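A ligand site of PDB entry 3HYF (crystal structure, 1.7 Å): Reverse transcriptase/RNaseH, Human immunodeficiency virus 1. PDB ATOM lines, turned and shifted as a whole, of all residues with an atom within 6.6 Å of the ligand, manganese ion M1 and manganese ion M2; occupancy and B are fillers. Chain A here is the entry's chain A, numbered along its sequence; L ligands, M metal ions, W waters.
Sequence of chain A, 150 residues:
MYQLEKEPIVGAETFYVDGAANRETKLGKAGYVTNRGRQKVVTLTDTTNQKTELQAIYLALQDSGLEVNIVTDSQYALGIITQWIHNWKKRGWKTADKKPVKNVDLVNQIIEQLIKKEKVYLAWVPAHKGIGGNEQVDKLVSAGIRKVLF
Merely in contact with the ligand: Ala 127 (3.6 Å), Leu 149 (3.8 Å), Lys 129 (3.9 Å) and Ser 74 (3.99 Å).
Hydrophobic or aromatic side chains that line the ligand: His 128 and Leu 149.
Of the 23 residues printed, 10 come within 4 Å of the ligand.
NH2 of Arg 146 is in salt-bridge range of OD1 of Asp 138, 2.9 Å away.
OD1 of Asp 73 sits at hydrogen-bond distance from ND2 of Asn 134 (2.9 Å).
O of Asp 73 sits at hydrogen-bond distance from NE1 of Trp 124.
OG of Ser 142 lies within hydrogen-bond range of O of Asp 138 (2.7 Å).
The side-chain hydroxyl (OG1) of Thr 72 lies within hydrogen-bond range of the backbone NH (N) of Ser 74.
The nearest printed residue that does not touch manganese ion M2 is Asp 73 (4.004 Å).
Manganese ion M2 is bound by the side-chain carboxylate (OD2) of Asp 18 (2.1 Å), the side-chain carboxylate (OD2) of Asp 138 (2.1 Å), water W6 (2.2 Å), water W2 (2.2 Å), an oxygen (O2) of the ligand (2.2 Å) and an oxygen (O1) of the ligand (2.2 Å).
Manganese ion M1 is bound by an oxygen (O1) of the ligand (2.1 Å), the side-chain carboxylate (OD2) of Asp 73 (2.1 Å), the side-chain carboxylate (OD1) of Asp 18 (2.1 Å), the side-chain carboxylate (OE1) of Glu 53 (2.1 Å) and an oxygen (O4) of the ligand (2.2 Å).
Manganese ion M1 has five donor atoms within binding distance.
Along chain A the residues within 4 Å of manganese ion M1 span positions 18 to 73.
The nearest printed residue that does not touch manganese ion M1 is Gly 19 (4.3 Å).
Water W7 lies within hydrogen-bond range of O3 of the ligand (2.7 Å), O of Asp 73 (2.8 Å) and N of Gln 75 (3.0 Å).
Water W8 bridges the side-chain hydroxyl of Ser 74 (2.7 Å) and an oxygen (O3) of the ligand (3.2 Å).
Water W3 lies within hydrogen-bond range of the backbone carbonyl oxygen (O) of Ala 127 (2.8 Å) and the side-chain amino group (NZ) of Lys 129 (3.2 Å).
A ring nitrogen (NE2) of His 128 sits close to a nitrogen (N2) of the ligand (3.4 Å).
The guanidinium group of Arg 146 sits close to an oxygen (O2) of the ligand (3.1 Å).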
ATOM      1  N   VAL A  17     -30.748   3.637 -16.960  1.00  0.00           N
ATOM      2  CA  VAL A  17     -30.718   4.974 -17.526  1.00  0.00           C
ATOM      3  C   VAL A  17     -30.303   4.914 -18.987  1.00  0.00           C
ATOM      4  O   VAL A  17     -29.645   3.974 -19.416  1.00  0.00           O
ATOM      5  CB  VAL A  17     -29.758   5.903 -16.749  1.00  0.00           C
ATOM      6  CG1 VAL A  17     -30.298   6.122 -15.347  1.00  0.00           C
ATOM      7  CG2 VAL A  17     -28.338   5.328 -16.718  1.00  0.00           C
ATOM      8  N   ASP A  18     -30.702   5.930 -19.756  1.00  0.00           N
ATOM      9  CA  ASP A  18     -30.156   6.063 -21.105  1.00  0.00           C
ATOM     10  C   ASP A  18     -30.475   7.436 -21.636  1.00  0.00           C
ATOM     11  O   ASP A  18     -31.293   8.156 -21.067  1.00  0.00           O
ATOM     12  CB  ASP A  18     -30.760   5.000 -22.026  1.00  0.00           C
ATOM     13  CG  ASP A  18     -29.903   4.771 -23.279  1.00  0.00           C
ATOM     14  OD1 ASP A  18     -28.707   5.122 -23.265  1.00  0.00           O
ATOM     15  OD2 ASP A  18     -30.438   4.243 -24.267  1.00  0.00           O
ATOM     16  N   GLY A  19     -29.801   7.798 -22.726  1.00  0.00           N
ATOM     17  CA  GLY A  19     -30.102   9.048 -23.377  1.00  0.00           C
ATOM     18  C   GLY A  19     -29.959   8.862 -24.875  1.00  0.00           C
ATOM     19  O   GLY A  19     -29.299   7.930 -25.332  1.00  0.00           O
ATOM     20  N   ALA A  20     -30.593   9.754 -25.630  1.00  0.00           N
ATOM     21  CA  ALA A  20     -30.476   9.748 -27.091  1.00  0.00           C
ATOM     22  C   ALA A  20     -30.503  11.192 -27.567  1.00  0.00           C
ATOM     23  O   ALA A  20     -31.180  12.041 -26.980  1.00  0.00           O
ATOM     24  CB  ALA A  20     -31.643   8.978 -27.704  1.00  0.00           C
ATOM     25  N   GLU A  53     -26.641  11.154 -21.629  1.00  0.00           N
ATOM     26  CA  GLU A  53     -26.312  10.026 -20.736  1.00  0.00           C
ATOM     27  C   GLU A  53     -25.966  10.520 -19.332  1.00  0.00           C
ATOM     28  O   GLU A  53     -26.365   9.897 -18.347  1.00  0.00           O
ATOM     29  CB  GLU A  53     -25.134   9.211 -21.282  1.00  0.00           C
ATOM     30  CG  GLU A  53     -25.375   8.614 -22.645  1.00  0.00           C
ATOM     31  CD  GLU A  53     -26.120   7.286 -22.629  1.00  0.00           C
ATOM     32  OE1 GLU A  53     -26.303   6.708 -23.717  1.00  0.00           O
ATOM     33  OE2 GLU A  53     -26.534   6.812 -21.541  1.00  0.00           O
ATOM     34  N   THR A  72     -26.104   1.760 -16.380  1.00  0.00           N
ATOM     35  CA  THR A  72     -25.922   2.580 -17.584  1.00  0.00           C
ATOM     36  C   THR A  72     -25.350   1.690 -18.688  1.00  0.00           C
ATOM     37  O   THR A  72     -24.719   0.663 -18.413  1.00  0.00           O
ATOM     38  CB  THR A  72     -24.951   3.757 -17.304  1.00  0.00           C
ATOM     39  OG1 THR A  72     -24.804   4.570 -18.484  1.00  0.00           O
ATOM     40  CG2 THR A  72     -23.566   3.255 -16.865  1.00  0.00           C
ATOM     41  N   ASP A  73     -25.574   2.080 -19.945  1.00  0.00           N
ATOM     42  CA  ASP A  73     -24.871   1.442 -21.059  1.00  0.00           C
ATOM     43  C   ASP A  73     -23.853   2.367 -21.694  1.00  0.00           C
ATOM     44  O   ASP A  73     -23.274   2.054 -22.743  1.00  0.00           O
ATOM     45  CB  ASP A  73     -25.861   0.893 -22.108  1.00  0.00           C
ATOM     46  CG  ASP A  73     -26.683   1.985 -22.801  1.00  0.00           C
ATOM     47  OD1 ASP A  73     -27.767   1.673 -23.313  1.00  0.00           O
ATOM     48  OD2 ASP A  73     -26.237   3.141 -22.819  1.00  0.00           O
ATOM     49  N   SER A  74     -23.595   3.506 -21.040  1.00  0.00           N
ATOM     50  CA  SER A  74     -22.690   4.506 -21.575  1.00  0.00           C
ATOM     51  C   SER A  74     -21.258   4.308 -21.099  1.00  0.00           C
ATOM     52  O   SER A  74     -20.940   4.549 -19.938  1.00  0.00           O
ATOM     53  CB  SER A  74     -23.158   5.901 -21.179  1.00  0.00           C
ATOM     54  OG  SER A  74     -22.262   6.885 -21.678  1.00  0.00           O
ATOM     55  N   GLN A  75     -20.381   3.901 -22.014  1.00  0.00           N
ATOM     56  CA  GLN A  75     -18.971   3.751 -21.671  1.00  0.00           C
ATOM     57  C   GLN A  75     -18.387   5.103 -21.266  1.00  0.00           C
ATOM     58  O   GLN A  75     -17.590   5.177 -20.342  1.00  0.00           O
ATOM     59  CB  GLN A  75     -18.187   3.182 -22.847  1.00  0.00           C
ATOM     60  CG  GLN A  75     -18.576   1.743 -23.183  1.00  0.00           C
ATOM     61  CD  GLN A  75     -17.840   1.234 -24.398  1.00  0.00           C
ATOM     62  OE1 GLN A  75     -17.990   1.768 -25.499  1.00  0.00           O
ATOM     63  NE2 GLN A  75     -17.035   0.188 -24.213  1.00  0.00           N
ATOM     64  N   TYR A  76     -18.779   6.159 -21.966  1.00  0.00           N
ATOM     65  CA  TYR A  76     -18.305   7.495 -21.622  1.00  0.00           C
ATOM     66  C   TYR A  76     -18.731   7.893 -20.204  1.00  0.00           C
ATOM     67  O   TYR A  76     -17.898   8.258 -19.387  1.00  0.00           O
ATOM     68  CB  TYR A  76     -18.837   8.517 -22.629  1.00  0.00           C
ATOM     69  CG  TYR A  76     -18.713   9.949 -22.166  1.00  0.00           C
ATOM     70  CD1 TYR A  76     -17.487  10.604 -22.171  1.00  0.00           C
ATOM     71  CD2 TYR A  76     -19.819  10.645 -21.695  1.00  0.00           C
ATOM     72  CE1 TYR A  76     -17.369  11.903 -21.731  1.00  0.00           C
ATOM     73  CE2 TYR A  76     -19.711  11.957 -21.249  1.00  0.00           C
ATOM     74  CZ  TYR A  76     -18.476  12.580 -21.272  1.00  0.00           C
ATOM     75  OH  TYR A  76     -18.354  13.875 -20.819  1.00  0.00           O
ATOM     76  N   TRP A 124     -22.169  -1.048 -15.682  1.00  0.00           N
ATOM     77  CA  TRP A 124     -22.311  -0.909 -17.125  1.00  0.00           C
ATOM     78  C   TRP A 124     -22.837  -2.194 -17.707  1.00  0.00           C
ATOM     79  O   TRP A 124     -22.451  -3.283 -17.287  1.00  0.00           O
ATOM     80  CB  TRP A 124     -20.954  -0.593 -17.755  1.00  0.00           C
ATOM     81  CG  TRP A 124     -21.000  -0.473 -19.234  1.00  0.00           C
ATOM     82  CD1 TRP A 124     -21.341   0.628 -19.961  1.00  0.00           C
ATOM     83  CD2 TRP A 124     -20.704  -1.508 -20.180  1.00  0.00           C
ATOM     84  NE1 TRP A 124     -21.271   0.345 -21.308  1.00  0.00           N
ATOM     85  CE2 TRP A 124     -20.887  -0.958 -21.465  1.00  0.00           C
ATOM     86  CE3 TRP A 124     -20.302  -2.842 -20.068  1.00  0.00           C
ATOM     87  CZ2 TRP A 124     -20.672  -1.692 -22.632  1.00  0.00           C
ATOM     88  CZ3 TRP A 124     -20.094  -3.571 -21.224  1.00  0.00           C
ATOM     89  CH2 TRP A 124     -20.283  -2.998 -22.486  1.00  0.00           C
ATOM     90  N   PRO A 126     -23.945  -3.757 -21.864  1.00  0.00           N
ATOM     91  CA  PRO A 126     -23.911  -3.409 -23.289  1.00  0.00           C
ATOM     92  C   PRO A 126     -25.288  -3.058 -23.852  1.00  0.00           C
ATOM     93  O   PRO A 126     -26.268  -3.732 -23.579  1.00  0.00           O
ATOM     94  CB  PRO A 126     -23.321  -4.659 -23.939  1.00  0.00           C
ATOM     95  CG  PRO A 126     -23.690  -5.774 -22.999  1.00  0.00           C
ATOM     96  CD  PRO A 126     -23.641  -5.177 -21.614  1.00  0.00           C
ATOM     97  N   ALA A 127     -25.324  -1.992 -24.653  1.00  0.00           N
ATOM     98  CA  ALA A 127     -26.553  -1.534 -25.283  1.00  0.00           C
ATOM     99  C   ALA A 127     -27.076  -2.541 -26.307  1.00  0.00           C
ATOM    100  O   ALA A 127     -26.287  -3.204 -26.990  1.00  0.00           O
ATOM    101  CB  ALA A 127     -26.319  -0.193 -25.972  1.00  0.00           C
ATOM    102  N   HIS A 128     -28.397  -2.637 -26.418  1.00  0.00           N
ATOM    103  CA  HIS A 128     -29.063  -3.443 -27.440  1.00  0.00           C
ATOM    104  C   HIS A 128     -28.665  -4.915 -27.384  1.00  0.00           C
ATOM    105  O   HIS A 128     -28.431  -5.543 -28.417  1.00  0.00           O
ATOM    106  CB  HIS A 128     -28.774  -2.843 -28.808  1.00  0.00           C
ATOM    107  CG  HIS A 128     -29.285  -1.438 -28.951  1.00  0.00           C
ATOM    108  ND1 HIS A 128     -30.628  -1.150 -29.023  1.00  0.00           N
ATOM    109  CD2 HIS A 128     -28.639  -0.248 -28.918  1.00  0.00           C
ATOM    110  CE1 HIS A 128     -30.799   0.161 -29.030  1.00  0.00           C
ATOM    111  NE2 HIS A 128     -29.610   0.735 -28.974  1.00  0.00           N
ATOM    112  N   LYS A 129     -28.587  -5.435 -26.166  1.00  0.00           N
ATOM    113  CA  LYS A 129     -28.267  -6.844 -25.963  1.00  0.00           C
ATOM    114  C   LYS A 129     -29.352  -7.521 -25.156  1.00  0.00           C
ATOM    115  O   LYS A 129     -29.115  -8.544 -24.513  1.00  0.00           O
ATOM    116  CB  LYS A 129     -26.917  -6.985 -25.249  1.00  0.00           C
ATOM    117  CG  LYS A 129     -25.715  -6.683 -26.124  1.00  0.00           C
ATOM    118  CD  LYS A 129     -25.524  -7.755 -27.191  1.00  0.00           C
ATOM    119  CE  LYS A 129     -25.619  -7.181 -28.596  1.00  0.00           C
ATOM    120  NZ  LYS A 129     -24.501  -6.246 -28.886  1.00  0.00           N
ATOM    121  N   ASN A 134     -32.819  -1.990 -19.637  1.00  0.00           N
ATOM    122  CA  ASN A 134     -32.048  -1.175 -20.579  1.00  0.00           C
ATOM    123  C   ASN A 134     -32.787  -0.994 -21.908  1.00  0.00           C
ATOM    124  O   ASN A 134     -32.828   0.106 -22.464  1.00  0.00           O
ATOM    125  CB  ASN A 134     -30.685  -1.827 -20.800  1.00  0.00           C
ATOM    126  CG  ASN A 134     -29.896  -1.160 -21.905  1.00  0.00           C
ATOM    127  OD1 ASN A 134     -29.917  -1.620 -23.045  1.00  0.00           O
ATOM    128  ND2 ASN A 134     -29.215  -0.073 -21.572  1.00  0.00           N
ATOM    129  N   VAL A 137     -35.712   1.579 -21.367  1.00  0.00           N
ATOM    130  CA  VAL A 137     -35.405   2.993 -21.286  1.00  0.00           C
ATOM    131  C   VAL A 137     -34.859   3.496 -22.628  1.00  0.00           C
ATOM    132  O   VAL A 137     -35.115   4.623 -23.019  1.00  0.00           O
ATOM    133  CB  VAL A 137     -34.415   3.324 -20.124  1.00  0.00           C
ATOM    134  CG1 VAL A 137     -33.056   2.646 -20.328  1.00  0.00           C
ATOM    135  CG2 VAL A 137     -34.247   4.832 -20.022  1.00  0.00           C
ATOM    136  N   ASP A 138     -34.115   2.650 -23.342  1.00  0.00           N
ATOM    137  CA  ASP A 138     -33.659   3.059 -24.664  1.00  0.00           C
ATOM    138  C   ASP A 138     -34.828   3.382 -25.596  1.00  0.00           C
ATOM    139  O   ASP A 138     -34.778   4.357 -26.347  1.00  0.00           O
ATOM    140  CB  ASP A 138     -32.775   1.977 -25.296  1.00  0.00           C
ATOM    141  CG  ASP A 138     -32.476   2.265 -26.758  1.00  0.00           C
ATOM    142  OD1 ASP A 138     -33.209   1.764 -27.632  1.00  0.00           O
ATOM    143  OD2 ASP A 138     -31.501   2.997 -27.030  1.00  0.00           O
ATOM    144  N   LYS A 139     -35.879   2.564 -25.541  1.00  0.00           N
ATOM    145  CA  LYS A 139     -37.055   2.825 -26.371  1.00  0.00           C
ATOM    146  C   LYS A 139     -37.684   4.174 -26.005  1.00  0.00           C
ATOM    147  O   LYS A 139     -38.110   4.937 -26.872  1.00  0.00           O
ATOM    148  CB  LYS A 139     -38.086   1.702 -26.200  1.00  0.00           C
ATOM    149  CG  LYS A 139     -39.347   1.873 -27.026  1.00  0.00           C
ATOM    150  CD  LYS A 139     -40.235   0.647 -26.931  1.00  0.00           C
ATOM    151  CE  LYS A 139     -41.461   0.772 -27.833  1.00  0.00           C
ATOM    152  NZ  LYS A 139     -42.304   1.935 -27.467  1.00  0.00           N
ATOM    153  N   VAL A 141     -36.216   6.975 -24.603  1.00  0.00           N
ATOM    154  CA  VAL A 141     -35.481   8.186 -24.942  1.00  0.00           C
ATOM    155  C   VAL A 141     -35.232   8.303 -26.452  1.00  0.00           C
ATOM    156  O   VAL A 141     -34.938   9.385 -26.943  1.00  0.00           O
ATOM    157  CB  VAL A 141     -34.119   8.269 -24.193  1.00  0.00           C
ATOM    158  CG1 VAL A 141     -34.373   8.210 -22.682  1.00  0.00           C
ATOM    159  CG2 VAL A 141     -33.169   7.157 -24.640  1.00  0.00           C
ATOM    160  N   SER A 142     -35.376   7.204 -27.170  1.00  0.00           N
ATOM    161  CA  SER A 142     -35.095   7.222 -28.600  1.00  0.00           C
ATOM    162  C   SER A 142     -36.324   7.605 -29.399  1.00  0.00           C
ATOM    163  O   SER A 142     -36.215   8.057 -30.534  1.00  0.00           O
ATOM    164  CB  SER A 142     -34.567   5.860 -29.068  1.00  0.00           C
ATOM    165  OG  SER A 142     -35.544   4.854 -28.923  1.00  0.00           O
ATOM    166  N   ARG A 146     -34.419   9.090 -32.375  1.00  0.00           N
ATOM    167  CA  ARG A 146     -33.611   8.238 -33.232  1.00  0.00           C
ATOM    168  C   ARG A 146     -34.502   7.570 -34.264  1.00  0.00           C
ATOM    169  O   ARG A 146     -35.401   6.801 -33.926  1.00  0.00           O
ATOM    170  CB  ARG A 146     -32.877   7.163 -32.408  1.00  0.00           C
ATOM    171  CG  ARG A 146     -31.904   6.326 -33.229  1.00  0.00           C
ATOM    172  CD  ARG A 146     -31.237   5.245 -32.386  1.00  0.00           C
ATOM    173  NE  ARG A 146     -32.207   4.242 -31.930  1.00  0.00           N
ATOM    174  CZ  ARG A 146     -32.192   3.687 -30.724  1.00  0.00           C
ATOM    175  NH1 ARG A 146     -31.255   4.016 -29.849  1.00  0.00           N
ATOM    176  NH2 ARG A 146     -33.114   2.802 -30.391  1.00  0.00           N
ATOM    177  N   LEU A 149     -32.539   2.062 -35.553  1.00  0.00           N
ATOM    178  CA  LEU A 149     -31.341   1.593 -34.849  1.00  0.00           C
ATOM    179  C   LEU A 149     -30.231   1.260 -35.842  1.00  0.00           C
ATOM    180  O   LEU A 149     -30.548   1.040 -37.029  1.00  0.00           O
ATOM    181  CB  LEU A 149     -31.686   0.358 -34.007  1.00  0.00           C
ATOM    182  CG  LEU A 149     -30.573  -0.167 -33.115  1.00  0.00           C
ATOM    183  CD1 LEU A 149     -30.067   0.946 -32.226  1.00  0.00           C
ATOM    184  CD2 LEU A 149     -31.076  -1.335 -32.291  1.00  0.00           C
HETATM  185  C1  LIG L   1     -25.904   0.375 -31.892  1.00  0.00           C
HETATM  186  N1  LIG L   1     -24.802   3.185 -28.235  1.00  0.00           N
HETATM  187  O1  LIG L   1     -27.562   4.128 -25.875  1.00  0.00           O
HETATM  188 CL1  LIG L   1     -26.027  -3.720 -31.375  1.00  0.00          CL
HETATM  189  C2  LIG L   1     -26.172  -1.007 -32.122  1.00  0.00           C
HETATM  190  N2  LIG L   1     -26.932   2.733 -29.221  1.00  0.00           N
HETATM  191  O2  LIG L   1     -28.877   3.184 -28.082  1.00  0.00           O
HETATM  192 CL2  LIG L   1     -27.019  -1.405 -33.566  1.00  0.00          CL
HETATM  193  C3  LIG L   1     -25.736  -2.028 -31.153  1.00  0.00           C
HETATM  194  O3  LIG L   1     -23.209   4.032 -26.322  1.00  0.00           O
HETATM  195  C4  LIG L   1     -25.026  -1.622 -29.960  1.00  0.00           C
HETATM  196  O4  LIG L   1     -24.796   4.594 -24.964  1.00  0.00           O
HETATM  197  C5  LIG L   1     -24.752  -0.235 -29.746  1.00  0.00           C
HETATM  198  C6  LIG L   1     -25.182   0.775 -30.697  1.00  0.00           C
HETATM  199  C7  LIG L   1     -24.886   2.242 -30.455  1.00  0.00           C
HETATM  200  C8  LIG L   1     -25.589   2.751 -29.235  1.00  0.00           C
HETATM  201  C9  LIG L   1     -25.405   3.674 -27.074  1.00  0.00           C
HETATM  202  C10 LIG L   1     -26.855   3.692 -26.949  1.00  0.00           C
HETATM  203  C11 LIG L   1     -27.560   3.205 -28.080  1.00  0.00           C
HETATM  204  C12 LIG L   1     -24.421   4.131 -26.039  1.00  0.00           C
HETATM  205 MN    MN M   1     -26.817   4.698 -24.045  1.00  0.00          MN
HETATM  206 MN    MN M   2     -29.698   3.745 -26.143  1.00  0.00          MN
HETATM  207  O   HOH W   1     -28.193   3.964 -31.554  1.00  0.00           O
HETATM  208  O   HOH W   2     -29.212   1.731 -25.485  1.00  0.00           O
HETATM  209  O   HOH W   3     -23.548  -3.575 -27.461  1.00  0.00           O
HETATM  210  O   HOH W   4     -28.819   6.300 -29.266  1.00  0.00           O
HETATM  211  O   HOH W   5     -26.089   6.728 -28.382  1.00  0.00           O
HETATM  212  O   HOH W   6     -30.012   5.736 -26.899  1.00  0.00           O
HETATM  213  O   HOH W   7     -21.407   2.948 -24.633  1.00  0.00           O
HETATM  214  O   HOH W   8     -22.865   6.540 -24.312  1.00  0.00           O
HETATM  215  O   HOH W   9     -20.831   4.854 -28.275  1.00  0.00           O
HETATM  216  O   HOH W  10     -22.010   2.266 -28.551  1.00  0.00           O
HETATM  217  O   HOH W  11     -24.870   5.705 -30.460  1.00  0.00           O
